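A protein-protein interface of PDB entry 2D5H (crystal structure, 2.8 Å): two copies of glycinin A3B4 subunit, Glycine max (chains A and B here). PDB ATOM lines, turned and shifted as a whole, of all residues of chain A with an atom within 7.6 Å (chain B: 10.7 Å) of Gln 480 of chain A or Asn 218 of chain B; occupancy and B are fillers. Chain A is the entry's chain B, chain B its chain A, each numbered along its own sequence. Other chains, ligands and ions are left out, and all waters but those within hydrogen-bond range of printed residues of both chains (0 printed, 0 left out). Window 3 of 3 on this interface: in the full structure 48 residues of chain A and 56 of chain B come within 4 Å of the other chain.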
ATOM      1  N   LYS A 456      15.685   0.507  35.779  1.00  0.00           N
ATOM      2  CA  LYS A 456      16.485  -0.179  34.775  1.00  0.00           C
ATOM      3  C   LYS A 456      16.757  -1.628  35.158  1.00  0.00           C
ATOM      4  O   LYS A 456      16.567  -2.532  34.348  1.00  0.00           O
ATOM      5  CB  LYS A 456      17.811   0.555  34.553  1.00  0.00           C
ATOM      6  CG  LYS A 456      18.657  -0.041  33.435  1.00  0.00           C
ATOM      7  CD  LYS A 456      19.866   0.826  33.106  1.00  0.00           C
ATOM      8  CE  LYS A 456      20.850   0.903  34.262  1.00  0.00           C
ATOM      9  NZ  LYS A 456      22.045   1.721  33.904  1.00  0.00           N
ATOM     10  N   LEU A 473       6.995  -0.380  22.305  1.00  0.00           N
ATOM     11  CA  LEU A 473       8.318  -0.322  21.695  1.00  0.00           C
ATOM     12  C   LEU A 473       8.503  -1.501  20.745  1.00  0.00           C
ATOM     13  O   LEU A 473       7.644  -2.380  20.657  1.00  0.00           O
ATOM     14  CB  LEU A 473       9.408  -0.366  22.775  1.00  0.00           C
ATOM     15  CG  LEU A 473       9.461   0.734  23.841  1.00  0.00           C
ATOM     16  CD1 LEU A 473      10.574   0.418  24.832  1.00  0.00           C
ATOM     17  CD2 LEU A 473       9.696   2.088  23.190  1.00  0.00           C
ATOM     18  N   GLY A 474       9.626  -1.513  20.033  1.00  0.00           N
ATOM     19  CA  GLY A 474       9.911  -2.599  19.112  1.00  0.00           C
ATOM     20  C   GLY A 474      11.136  -3.355  19.586  1.00  0.00           C
ATOM     21  O   GLY A 474      11.805  -2.912  20.520  1.00  0.00           O
ATOM     22  N   GLN A 475      11.437  -4.486  18.953  1.00  0.00           N
ATOM     23  CA  GLN A 475      12.597  -5.287  19.338  1.00  0.00           C
ATOM     24  C   GLN A 475      13.867  -4.443  19.428  1.00  0.00           C
ATOM     25  O   GLN A 475      14.827  -4.820  20.102  1.00  0.00           O
ATOM     26  CB  GLN A 475      12.811  -6.432  18.345  1.00  0.00           C
ATOM     27  CG  GLN A 475      14.052  -7.273  18.630  1.00  0.00           C
ATOM     28  CD  GLN A 475      14.065  -7.837  20.041  1.00  0.00           C
ATOM     29  OE1 GLN A 475      13.219  -8.658  20.403  1.00  0.00           O
ATOM     30  NE2 GLN A 475      15.024  -7.394  20.849  1.00  0.00           N
ATOM     31  N   SER A 476      13.870  -3.304  18.744  1.00  0.00           N
ATOM     32  CA  SER A 476      15.019  -2.407  18.761  1.00  0.00           C
ATOM     33  C   SER A 476      15.033  -1.598  20.057  1.00  0.00           C
ATOM     34  O   SER A 476      15.986  -1.670  20.834  1.00  0.00           O
ATOM     35  CB  SER A 476      14.971  -1.459  17.557  1.00  0.00           C
ATOM     36  OG  SER A 476      13.781  -0.689  17.555  1.00  0.00           O
ATOM     37  N   GLN A 477      13.968  -0.837  20.286  1.00  0.00           N
ATOM     38  CA  GLN A 477      13.852  -0.014  21.485  1.00  0.00           C
ATOM     39  C   GLN A 477      13.796  -0.871  22.746  1.00  0.00           C
ATOM     40  O   GLN A 477      14.284  -0.470  23.803  1.00  0.00           O
ATOM     41  CB  GLN A 477      12.603   0.866  21.404  1.00  0.00           C
ATOM     42  CG  GLN A 477      12.607   1.836  20.239  1.00  0.00           C
ATOM     43  CD  GLN A 477      11.457   2.820  20.300  1.00  0.00           C
ATOM     44  OE1 GLN A 477      10.290   2.432  20.270  1.00  0.00           O
ATOM     45  NE2 GLN A 477      11.782   4.103  20.391  1.00  0.00           N
ATOM     46  N   VAL A 478      13.190  -2.047  22.634  1.00  0.00           N
ATOM     47  CA  VAL A 478      13.090  -2.950  23.772  1.00  0.00           C
ATOM     48  C   VAL A 478      14.482  -3.464  24.105  1.00  0.00           C
ATOM     49  O   VAL A 478      14.975  -3.268  25.216  1.00  0.00           O
ATOM     50  CB  VAL A 478      12.163  -4.143  23.462  1.00  0.00           C
ATOM     51  CG1 VAL A 478      12.252  -5.180  24.575  1.00  0.00           C
ATOM     52  CG2 VAL A 478      10.725  -3.653  23.310  1.00  0.00           C
ATOM     53  N   ARG A 479      15.117  -4.116  23.136  1.00  0.00           N
ATOM     54  CA  ARG A 479      16.461  -4.639  23.334  1.00  0.00           C
ATOM     55  C   ARG A 479      17.376  -3.476  23.698  1.00  0.00           C
ATOM     56  O   ARG A 479      18.421  -3.662  24.320  1.00  0.00           O
ATOM     57  CB  ARG A 479      16.963  -5.328  22.060  1.00  0.00           C
ATOM     58  CG  ARG A 479      18.369  -5.902  22.174  1.00  0.00           C
ATOM     59  CD  ARG A 479      18.526  -6.732  23.442  1.00  0.00           C
ATOM     60  NE  ARG A 479      19.828  -7.389  23.523  1.00  0.00           N
ATOM     61  CZ  ARG A 479      20.201  -8.409  22.757  1.00  0.00           C
ATOM     62  NH1 ARG A 479      19.372  -8.897  21.846  1.00  0.00           N
ATOM     63  NH2 ARG A 479      21.406  -8.943  22.905  1.00  0.00           N
ATOM     64  N   GLN A 480      16.969  -2.274  23.304  1.00  0.00           N
ATOM     65  CA  GLN A 480      17.732  -1.071  23.603  1.00  0.00           C
ATOM     66  C   GLN A 480      17.954  -1.009  25.109  1.00  0.00           C
ATOM     67  O   GLN A 480      19.070  -1.188  25.593  1.00  0.00           O
ATOM     68  CB  GLN A 480      16.957   0.172  23.141  1.00  0.00           C
ATOM     69  CG  GLN A 480      17.513   1.509  23.631  1.00  0.00           C
ATOM     70  CD  GLN A 480      18.764   1.953  22.888  1.00  0.00           C
ATOM     71  OE1 GLN A 480      19.383   2.957  23.245  1.00  0.00           O
ATOM     72  NE2 GLN A 480      19.135   1.215  21.847  1.00  0.00           N
ATOM     73  N   LEU A 481      16.870  -0.778  25.841  1.00  0.00           N
ATOM     74  CA  LEU A 481      16.918  -0.675  27.291  1.00  0.00           C
ATOM     75  C   LEU A 481      17.467  -1.930  27.966  1.00  0.00           C
ATOM     76  O   LEU A 481      18.379  -1.851  28.787  1.00  0.00           O
ATOM     77  CB  LEU A 481      15.519  -0.369  27.827  1.00  0.00           C
ATOM     78  CG  LEU A 481      14.780   0.750  27.088  1.00  0.00           C
ATOM     79  CD1 LEU A 481      13.478   1.063  27.813  1.00  0.00           C
ATOM     80  CD2 LEU A 481      15.658   1.993  27.005  1.00  0.00           C
ATOM     81  N   LYS A 482      16.915  -3.086  27.616  1.00  0.00           N
ATOM     82  CA  LYS A 482      17.352  -4.345  28.207  1.00  0.00           C
ATOM     83  C   LYS A 482      18.850  -4.583  28.016  1.00  0.00           C
ATOM     84  O   LYS A 482      19.492  -5.239  28.838  1.00  0.00           O
ATOM     85  CB  LYS A 482      16.558  -5.510  27.599  1.00  0.00           C
ATOM     86  CG  LYS A 482      15.047  -5.378  27.763  1.00  0.00           C
ATOM     87  CD  LYS A 482      14.266  -6.484  27.043  1.00  0.00           C
ATOM     88  CE  LYS A 482      14.374  -7.834  27.743  1.00  0.00           C
ATOM     89  NZ  LYS A 482      15.727  -8.436  27.633  1.00  0.00           N
ATOM     90  N   TYR A 483      19.403  -4.037  26.935  1.00  0.00           N
ATOM     91  CA  TYR A 483      20.823  -4.202  26.624  1.00  0.00           C
ATOM     92  C   TYR A 483      21.621  -2.943  26.958  1.00  0.00           C
ATOM     93  O   TYR A 483      22.443  -2.944  27.875  1.00  0.00           O
ATOM     94  CB  TYR A 483      20.994  -4.537  25.136  1.00  0.00           C
ATOM     95  CG  TYR A 483      22.389  -4.976  24.727  1.00  0.00           C
ATOM     96  CD1 TYR A 483      23.502  -4.168  24.969  1.00  0.00           C
ATOM     97  CD2 TYR A 483      22.591  -6.194  24.076  1.00  0.00           C
ATOM     98  CE1 TYR A 483      24.781  -4.561  24.572  1.00  0.00           C
ATOM     99  CE2 TYR A 483      23.865  -6.597  23.676  1.00  0.00           C
ATOM    100  CZ  TYR A 483      24.953  -5.775  23.927  1.00  0.00           C
ATOM    101  OH  TYR A 483      26.211  -6.165  23.530  1.00  0.00           O
ATOM    102  N   GLN A 484      21.379  -1.881  26.197  1.00  0.00           N
ATOM    103  CA  GLN A 484      22.069  -0.608  26.389  1.00  0.00           C
ATOM    104  C   GLN A 484      22.126  -0.196  27.856  1.00  0.00           C
ATOM    105  O   GLN A 484      23.120   0.373  28.310  1.00  0.00           O
ATOM    106  CB  GLN A 484      21.388   0.488  25.563  1.00  0.00           C
ATOM    107  CG  GLN A 484      21.722   0.464  24.068  1.00  0.00           C
ATOM    108  CD  GLN A 484      21.477  -0.889  23.410  1.00  0.00           C
ATOM    109  OE1 GLN A 484      22.140  -1.878  23.726  1.00  0.00           O
ATOM    110  NE2 GLN A 484      20.523  -0.935  22.486  1.00  0.00           N
ATOM    111  N   GLY A 485      21.058  -0.489  28.592  1.00  0.00           N
ATOM    112  CA  GLY A 485      21.022  -0.149  30.004  1.00  0.00           C
ATOM    113  C   GLY A 485      21.983  -1.021  30.794  1.00  0.00           C
ATOM    114  O   GLY A 485      21.608  -2.087  31.289  1.00  0.00           O
ATOM    115  N   ASN A 486      23.230  -0.570  30.903  1.00  0.00           N
ATOM    116  CA  ASN A 486      24.257  -1.309  31.629  1.00  0.00           C
ATOM    117  C   ASN A 486      23.906  -1.451  33.108  1.00  0.00           C
ATOM    118  O   ASN A 486      23.499  -0.486  33.758  1.00  0.00           O
ATOM    119  CB  ASN A 486      25.618  -0.620  31.470  1.00  0.00           C
ATOM    120  CG  ASN A 486      25.589   0.839  31.887  1.00  0.00           C
ATOM    121  OD1 ASN A 486      24.783   1.625  31.386  1.00  0.00           O
ATOM    122  ND2 ASN A 486      26.478   1.210  32.802  1.00  0.00           N
ATOM    123  N   GLY A 488      23.726  -1.056  36.506  1.00  0.00           N
ATOM    124  CA  GLY A 488      24.288  -0.099  37.443  1.00  0.00           C
ATOM    125  C   GLY A 488      23.382   1.102  37.640  1.00  0.00           C
ATOM    126  O   GLY A 488      23.060   1.803  36.679  1.00  0.00           O
ATOM    127  N   VAL A 491      24.675   6.271  36.645  1.00  0.00           N
ATOM    128  CA  VAL A 491      24.883   6.531  35.226  1.00  0.00           C
ATOM    129  C   VAL A 491      25.560   7.876  34.993  1.00  0.00           C
ATOM    130  O   VAL A 491      25.196   8.885  35.602  1.00  0.00           O
ATOM    131  CB  VAL A 491      23.546   6.512  34.452  1.00  0.00           C
ATOM    132  CG1 VAL A 491      23.794   6.792  32.975  1.00  0.00           C
ATOM    133  CG2 VAL A 491      22.861   5.162  34.630  1.00  0.00           C
ATOM    134  N   ASN A 492      26.547   7.876  34.102  1.00  0.00           N
ATOM    135  CA  ASN A 492      27.296   9.080  33.764  1.00  0.00           C
ATOM    136  C   ASN A 492      26.944   9.571  32.359  1.00  0.00           C
ATOM    137  O   ASN A 492      27.551   9.149  31.374  1.00  0.00           O
ATOM    138  CB  ASN A 492      28.799   8.797  33.856  1.00  0.00           C
ATOM    139  CG  ASN A 492      29.219   7.589  33.033  1.00  0.00           C
ATOM    140  OD1 ASN A 492      28.736   6.478  33.247  1.00  0.00           O
ATOM    141  ND2 ASN A 492      30.125   7.804  32.087  1.00  0.00           N
ATOM    142  N   PRO A 493      25.955  10.475  32.252  1.00  0.00           N
ATOM    143  CA  PRO A 493      25.528  11.019  30.958  1.00  0.00           C
ATOM    144  C   PRO A 493      26.638  11.785  30.242  1.00  0.00           C
ATOM    145  O   PRO A 493      26.905  11.467  29.063  1.00  0.00           O
ATOM    146  CB  PRO A 493      24.346  11.911  31.336  1.00  0.00           C
ATOM    147  CG  PRO A 493      24.722  12.396  32.699  1.00  0.00           C
ATOM    148  CD  PRO A 493      25.227  11.128  33.355  1.00  0.00           C
ATOM    149  OXT PRO A 493      27.225  12.696  30.867  1.00  0.00           O
ATOM    150  N   SER B 110      15.854 -13.230  28.392  1.00  0.00           N
ATOM    151  CA  SER B 110      16.537 -13.007  29.663  1.00  0.00           C
ATOM    152  C   SER B 110      15.566 -12.498  30.726  1.00  0.00           C
ATOM    153  O   SER B 110      15.634 -11.341  31.146  1.00  0.00           O
ATOM    154  CB  SER B 110      17.675 -12.001  29.483  1.00  0.00           C
ATOM    155  OG  SER B 110      17.181 -10.755  29.023  1.00  0.00           O
ATOM    156  N   SER B 209      10.784  13.665  32.763  1.00  0.00           N
ATOM    157  CA  SER B 209      10.850  14.203  31.408  1.00  0.00           C
ATOM    158  C   SER B 209      11.764  13.326  30.554  1.00  0.00           C
ATOM    159  O   SER B 209      12.743  12.766  31.053  1.00  0.00           O
ATOM    160  CB  SER B 209      11.378  15.642  31.438  1.00  0.00           C
ATOM    161  OG  SER B 209      12.643  15.712  32.073  1.00  0.00           O
ATOM    162  N   LYS B 210      11.445  13.207  29.268  1.00  0.00           N
ATOM    163  CA  LYS B 210      12.243  12.377  28.375  1.00  0.00           C
ATOM    164  C   LYS B 210      13.722  12.717  28.436  1.00  0.00           C
ATOM    165  O   LYS B 210      14.566  11.855  28.207  1.00  0.00           O
ATOM    166  CB  LYS B 210      11.744  12.488  26.930  1.00  0.00           C
ATOM    167  CG  LYS B 210      11.693  13.894  26.365  1.00  0.00           C
ATOM    168  CD  LYS B 210      11.317  13.853  24.890  1.00  0.00           C
ATOM    169  CE  LYS B 210      11.085  15.242  24.328  1.00  0.00           C
ATOM    170  NZ  LYS B 210       9.920  15.902  24.976  1.00  0.00           N
ATOM    171  N   HIS B 211      14.033  13.972  28.750  1.00  0.00           N
ATOM    172  CA  HIS B 211      15.422  14.414  28.846  1.00  0.00           C
ATOM    173  C   HIS B 211      16.182  13.661  29.932  1.00  0.00           C
ATOM    174  O   HIS B 211      17.090  12.876  29.640  1.00  0.00           O
ATOM    175  CB  HIS B 211      15.482  15.916  29.132  1.00  0.00           C
ATOM    176  CG  HIS B 211      15.235  16.772  27.930  1.00  0.00           C
ATOM    177  ND1 HIS B 211      14.131  16.619  27.120  1.00  0.00           N
ATOM    178  CD2 HIS B 211      15.946  17.801  27.409  1.00  0.00           C
ATOM    179  CE1 HIS B 211      14.171  17.518  26.153  1.00  0.00           C
ATOM    180  NE2 HIS B 211      15.262  18.248  26.305  1.00  0.00           N
ATOM    181  N   PHE B 212      15.808  13.909  31.184  1.00  0.00           N
ATOM    182  CA  PHE B 212      16.454  13.261  32.319  1.00  0.00           C
ATOM    183  C   PHE B 212      16.340  11.750  32.170  1.00  0.00           C
ATOM    184  O   PHE B 212      17.268  11.013  32.503  1.00  0.00           O
ATOM    185  CB  PHE B 212      15.796  13.707  33.630  1.00  0.00           C
ATOM    186  CG  PHE B 212      16.639  13.450  34.854  1.00  0.00           C
ATOM    187  CD1 PHE B 212      17.006  12.155  35.209  1.00  0.00           C
ATOM    188  CD2 PHE B 212      17.073  14.510  35.647  1.00  0.00           C
ATOM    189  CE1 PHE B 212      17.795  11.917  36.333  1.00  0.00           C
ATOM    190  CE2 PHE B 212      17.861  14.285  36.772  1.00  0.00           C
ATOM    191  CZ  PHE B 212      18.223  12.985  37.117  1.00  0.00           C
ATOM    192  N   LEU B 213      15.196  11.304  31.655  1.00  0.00           N
ATOM    193  CA  LEU B 213      14.931   9.883  31.454  1.00  0.00           C
ATOM    194  C   LEU B 213      15.839   9.289  30.381  1.00  0.00           C
ATOM    195  O   LEU B 213      16.519   8.288  30.613  1.00  0.00           O
ATOM    196  CB  LEU B 213      13.465   9.678  31.067  1.00  0.00           C
ATOM    197  CG  LEU B 213      12.959   8.238  30.948  1.00  0.00           C
ATOM    198  CD1 LEU B 213      13.187   7.492  32.251  1.00  0.00           C
ATOM    199  CD2 LEU B 213      11.480   8.255  30.603  1.00  0.00           C
ATOM    200  N   ALA B 214      15.844   9.909  29.205  1.00  0.00           N
ATOM    201  CA  ALA B 214      16.678   9.441  28.105  1.00  0.00           C
ATOM    202  C   ALA B 214      18.126   9.371  28.567  1.00  0.00           C
ATOM    203  O   ALA B 214      18.897   8.527  28.112  1.00  0.00           O
ATOM    204  CB  ALA B 214      16.554  10.381  26.917  1.00  0.00           C
ATOM    205  N   GLN B 215      18.490  10.265  29.479  1.00  0.00           N
ATOM    206  CA  GLN B 215      19.847  10.305  30.003  1.00  0.00           C
ATOM    207  C   GLN B 215      20.079   9.221  31.056  1.00  0.00           C
ATOM    208  O   GLN B 215      21.085   8.512  31.013  1.00  0.00           O
ATOM    209  CB  GLN B 215      20.137  11.690  30.590  1.00  0.00           C
ATOM    210  CG  GLN B 215      20.137  12.806  29.552  1.00  0.00           C
ATOM    211  CD  GLN B 215      20.454  14.169  30.143  1.00  0.00           C
ATOM    212  OE1 GLN B 215      21.471  14.346  30.814  1.00  0.00           O
ATOM    213  NE2 GLN B 215      19.586  15.144  29.890  1.00  0.00           N
ATOM    214  N   SER B 216      19.144   9.088  31.992  1.00  0.00           N
ATOM    215  CA  SER B 216      19.256   8.089  33.051  1.00  0.00           C
ATOM    216  C   SER B 216      19.406   6.678  32.489  1.00  0.00           C
ATOM    217  O   SER B 216      20.234   5.896  32.963  1.00  0.00           O
ATOM    218  CB  SER B 216      18.028   8.141  33.968  1.00  0.00           C
ATOM    219  OG  SER B 216      17.947   9.376  34.658  1.00  0.00           O
ATOM    220  N   PHE B 217      18.601   6.359  31.480  1.00  0.00           N
ATOM    221  CA  PHE B 217      18.640   5.040  30.859  1.00  0.00           C
ATOM    222  C   PHE B 217      19.430   5.047  29.556  1.00  0.00           C
ATOM    223  O   PHE B 217      19.262   4.162  28.718  1.00  0.00           O
ATOM    224  CB  PHE B 217      17.218   4.535  30.596  1.00  0.00           C
ATOM    225  CG  PHE B 217      16.390   4.381  31.839  1.00  0.00           C
ATOM    226  CD1 PHE B 217      15.951   5.498  32.542  1.00  0.00           C
ATOM    227  CD2 PHE B 217      16.060   3.120  32.317  1.00  0.00           C
ATOM    228  CE1 PHE B 217      15.198   5.359  33.703  1.00  0.00           C
ATOM    229  CE2 PHE B 217      15.305   2.972  33.480  1.00  0.00           C
ATOM    230  CZ  PHE B 217      14.875   4.096  34.172  1.00  0.00           C
ATOM    231  N   ASN B 218      20.295   6.044  29.399  1.00  0.00           N
ATOM    232  CA  ASN B 218      21.127   6.183  28.207  1.00  0.00           C
ATOM    233  C   ASN B 218      20.431   5.750  26.916  1.00  0.00           C
ATOM    234  O   ASN B 218      20.855   4.797  26.259  1.00  0.00           O
ATOM    235  CB  ASN B 218      22.428   5.391  28.379  1.00  0.00           C
ATOM    236  CG  ASN B 218      22.188   3.904  28.573  1.00  0.00           C
ATOM    237  OD1 ASN B 218      21.606   3.479  29.574  1.00  0.00           O
ATOM    238  ND2 ASN B 218      22.637   3.103  27.611  1.00  0.00           N
ATOM    239  N   THR B 219      19.361   6.453  26.556  1.00  0.00           N
ATOM    240  CA  THR B 219      18.612   6.151  25.341  1.00  0.00           C
ATOM    241  C   THR B 219      18.151   7.440  24.666  1.00  0.00           C
ATOM    242  O   THR B 219      18.130   8.505  25.287  1.00  0.00           O
ATOM    243  CB  THR B 219      17.370   5.281  25.641  1.00  0.00           C
ATOM    244  OG1 THR B 219      16.687   4.980  24.416  1.00  0.00           O
ATOM    245  CG2 THR B 219      16.417   6.014  26.577  1.00  0.00           C
ATOM    246  N   ASN B 220      17.779   7.334  23.394  1.00  0.00           N
ATOM    247  CA  ASN B 220      17.315   8.480  22.619  1.00  0.00           C
ATOM    248  C   ASN B 220      16.118   9.173  23.267  1.00  0.00           C
ATOM    249  O   ASN B 220      15.661   8.774  24.338  1.00  0.00           O
ATOM    250  CB  ASN B 220      16.949   8.027  21.203  1.00  0.00           C
ATOM    251  CG  ASN B 220      15.997   6.845  21.200  1.00  0.00           C
ATOM    252  OD1 ASN B 220      14.844   6.961  21.614  1.00  0.00           O
ATOM    253  ND2 ASN B 220      16.480   5.696  20.738  1.00  0.00           N
ATOM    254  N   GLU B 221      15.613  10.213  22.611  1.00  0.00           N
ATOM    255  CA  GLU B 221      14.475  10.963  23.127  1.00  0.00           C
ATOM    256  C   GLU B 221      13.175  10.368  22.604  1.00  0.00           C
ATOM    257  O   GLU B 221      12.098  10.922  22.823  1.00  0.00           O
ATOM    258  CB  GLU B 221      14.560  12.431  22.695  1.00  0.00           C
ATOM    259  CG  GLU B 221      15.962  13.009  22.719  1.00  0.00           C
ATOM    260  CD  GLU B 221      16.664  12.772  24.036  1.00  0.00           C
ATOM    261  OE1 GLU B 221      16.131  13.209  25.074  1.00  0.00           O
ATOM    262  OE2 GLU B 221      17.747  12.148  24.030  1.00  0.00           O
ATOM    263  N   ASP B 222      13.284   9.243  21.904  1.00  0.00           N
ATOM    264  CA  ASP B 222      12.116   8.572  21.345  1.00  0.00           C
ATOM    265  C   ASP B 222      11.652   7.454  22.274  1.00  0.00           C
ATOM    266  O   ASP B 222      10.533   7.486  22.787  1.00  0.00           O
ATOM    267  CB  ASP B 222      12.446   8.003  19.960  1.00  0.00           C
ATOM    268  CG  ASP B 222      11.255   7.319  19.307  1.00  0.00           C
ATOM    269  OD1 ASP B 222      10.189   7.962  19.192  1.00  0.00           O
ATOM    270  OD2 ASP B 222      11.384   6.143  18.907  1.00  0.00           O
ATOM    271  N   THR B 223      12.519   6.467  22.487  1.00  0.00           N
ATOM    272  CA  THR B 223      12.201   5.343  23.359  1.00  0.00           C
ATOM    273  C   THR B 223      11.750   5.871  24.715  1.00  0.00           C
ATOM    274  O   THR B 223      10.619   5.633  25.144  1.00  0.00           O
ATOM    275  CB  THR B 223      13.430   4.436  23.569  1.00  0.00           C
ATOM    276  OG1 THR B 223      13.915   3.986  22.296  1.00  0.00           O
ATOM    277  CG2 THR B 223      13.060   3.228  24.427  1.00  0.00           C
ATOM    278  N   ALA B 224      12.643   6.597  25.380  1.00  0.00           N
ATOM    279  CA  ALA B 224      12.352   7.171  26.685  1.00  0.00           C
ATOM    280  C   ALA B 224      11.065   7.987  26.643  1.00  0.00           C
ATOM    281  O   ALA B 224      10.335   8.064  27.633  1.00  0.00           O
ATOM    282  CB  ALA B 224      13.512   8.050  27.135  1.00  0.00           C
ATOM    283  N   GLU B 225      10.784   8.590  25.493  1.00  0.00           N
ATOM    284  CA  GLU B 225       9.583   9.404  25.340  1.00  0.00           C
ATOM    285  C   GLU B 225       8.334   8.532  25.445  1.00  0.00           C
ATOM    286  O   GLU B 225       7.338   8.929  26.055  1.00  0.00           O
ATOM    287  CB  GLU B 225       9.608  10.133  23.993  1.00  0.00           C
ATOM    288  CG  GLU B 225       8.812  11.427  23.976  1.00  0.00           C
ATOM    289  CD  GLU B 225       7.317  11.200  24.023  1.00  0.00           C
ATOM    290  OE1 GLU B 225       6.579  12.173  24.286  1.00  0.00           O
ATOM    291  OE2 GLU B 225       6.879  10.055  23.786  1.00  0.00           O
ATOM    292  N   LEU B 227       8.298   5.801  26.996  1.00  0.00           N
ATOM    293  CA  LEU B 227       8.361   5.248  28.346  1.00  0.00           C
ATOM    294  C   LEU B 227       7.483   6.034  29.317  1.00  0.00           C
ATOM    295  O   LEU B 227       7.215   5.583  30.430  1.00  0.00           O
ATOM    296  CB  LEU B 227       9.810   5.225  28.844  1.00  0.00           C
ATOM    297  CG  LEU B 227      10.756   4.265  28.111  1.00  0.00           C
ATOM    298  CD1 LEU B 227      12.172   4.414  28.649  1.00  0.00           C
ATOM    299  CD2 LEU B 227      10.268   2.834  28.286  1.00  0.00           C
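Of chain A, only Gln 480, Gln 484 and Gly 485 come within 4 Å of Asn 218 of chain B.
No residue of chain B comes within 4 Å of Ser 476 of chain A.
No residue of chain B comes within 4 Å of Val 478 of chain A.
Leu 481 of chain A touches just these residues of chain B: Thr 219 (3.9 Å), Thr 223 (3.9 Å) and Leu 227 (3.7 Å).
Of chain B, only Asn 218 comes within 4 Å of Gln 484 of chain A.
Of chain B, only Asn 218 (3.7 Å) comes within 4 Å of Gly 485 of chain A.
Printed residues of chain B within 4 Å of Val 491 of chain A: Gln 215 and Ser 216.
Printed residues of chain A within 4 Å of Thr 223 of chain B: Leu 473 (3.8 Å), Gln 477 (2.9 Å) and Leu 481 (3.9 Å).
Of the printed residues of chain B, Lys 456 of chain A touches Phe 217.
Ser 209 of chain B touches none of the printed residues of chain A.
The nearest printed residue of chain A that does not touch Phe 217 of chain B is Leu 481 of chain A (4.5 Å).
Phe 217 of chain B touches Lys 456 of chain A (CE2 to N, 3.4 Å).
OE1 of Gln 480 of chain A touches O of Asn 218 of chain B, 3.8 Å away.
Gln 480 of chain A touches Thr 219 of chain B.
Leu 481 of chain A touches Thr 219 of chain B.
CG2 of Thr 223 of chain B touches CD2 of Leu 481 of chain A (3.9 Å).
Leu 227 of chain B touches Leu 481 of chain A (CD1 to CD1, 3.7 Å).
Gly 485 of chain A touches Asn 218 of chain B.
Val 491 of chain A touches Gln 215 of chain B.
O of Ser 216 of chain B touches CG2 of Val 491 of chain A (3.2 Å).
Pro 493 of chain A touches Gln 215 of chain B (CB to OE1, 3.8 Å).
No position is printed for both chains.
The backbone NH (N) of Thr 219 of chain B sits at hydrogen-bond distance from the backbone carbonyl oxygen (O) of Ala 214 of chain B (2.6 Å).
OD1 of Asn 220 of chain B is in hydrogen-bond range of N of Asp 222 of chain B, 2.8 Å away.
The side-chain amide nitrogen (NE2) of Gln 484 of chain A lies close to the side-chain amide nitrogen (NE2) of Gln 480 of chain A.
The backbone NH (N) of Thr 223 of chain B lies within hydrogen-bond range of the side-chain amide oxygen (OD1) of Asn 220 of chain B.
The side-chain amino group (NZ) of Lys 456 of chain A sits at hydrogen-bond distance from the backbone carbonyl oxygen (O) of Gly 488 of chain A (3.0 Å).
O of His 211 of chain B sits close to NE2 of Gln 215 of chain B, 3.4 Å away.
Among the printed residues, 15 pairs touch across the chains.
Among the printed residues, no Asp or Glu carboxylate lies within 4 Å of a Lys or Arg side-chain nitrogen of the other chain.
The backbone carbonyl oxygen (O) of Gln 484 of chain A lies within hydrogen-bond range of the side-chain amide nitrogen (ND2) of Asn 218 of chain B (2.9 Å).
The side-chain amino group (NZ) of Lys 482 of chain A is in hydrogen-bond range of the side-chain hydroxyl (OG) of Ser 110 of chain B, 3.1 Å away.
The side-chain hydroxyl (OG1) of Thr 223 of chain B is in hydrogen-bond range of the side-chain amide nitrogen (NE2) of Gln 477 of chain A, at 2.9 Å.
OD2 of Asp 222 of chain B lies within hydrogen-bond range of NE2 of Gln 477 of chain A, at 2.6 Å.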
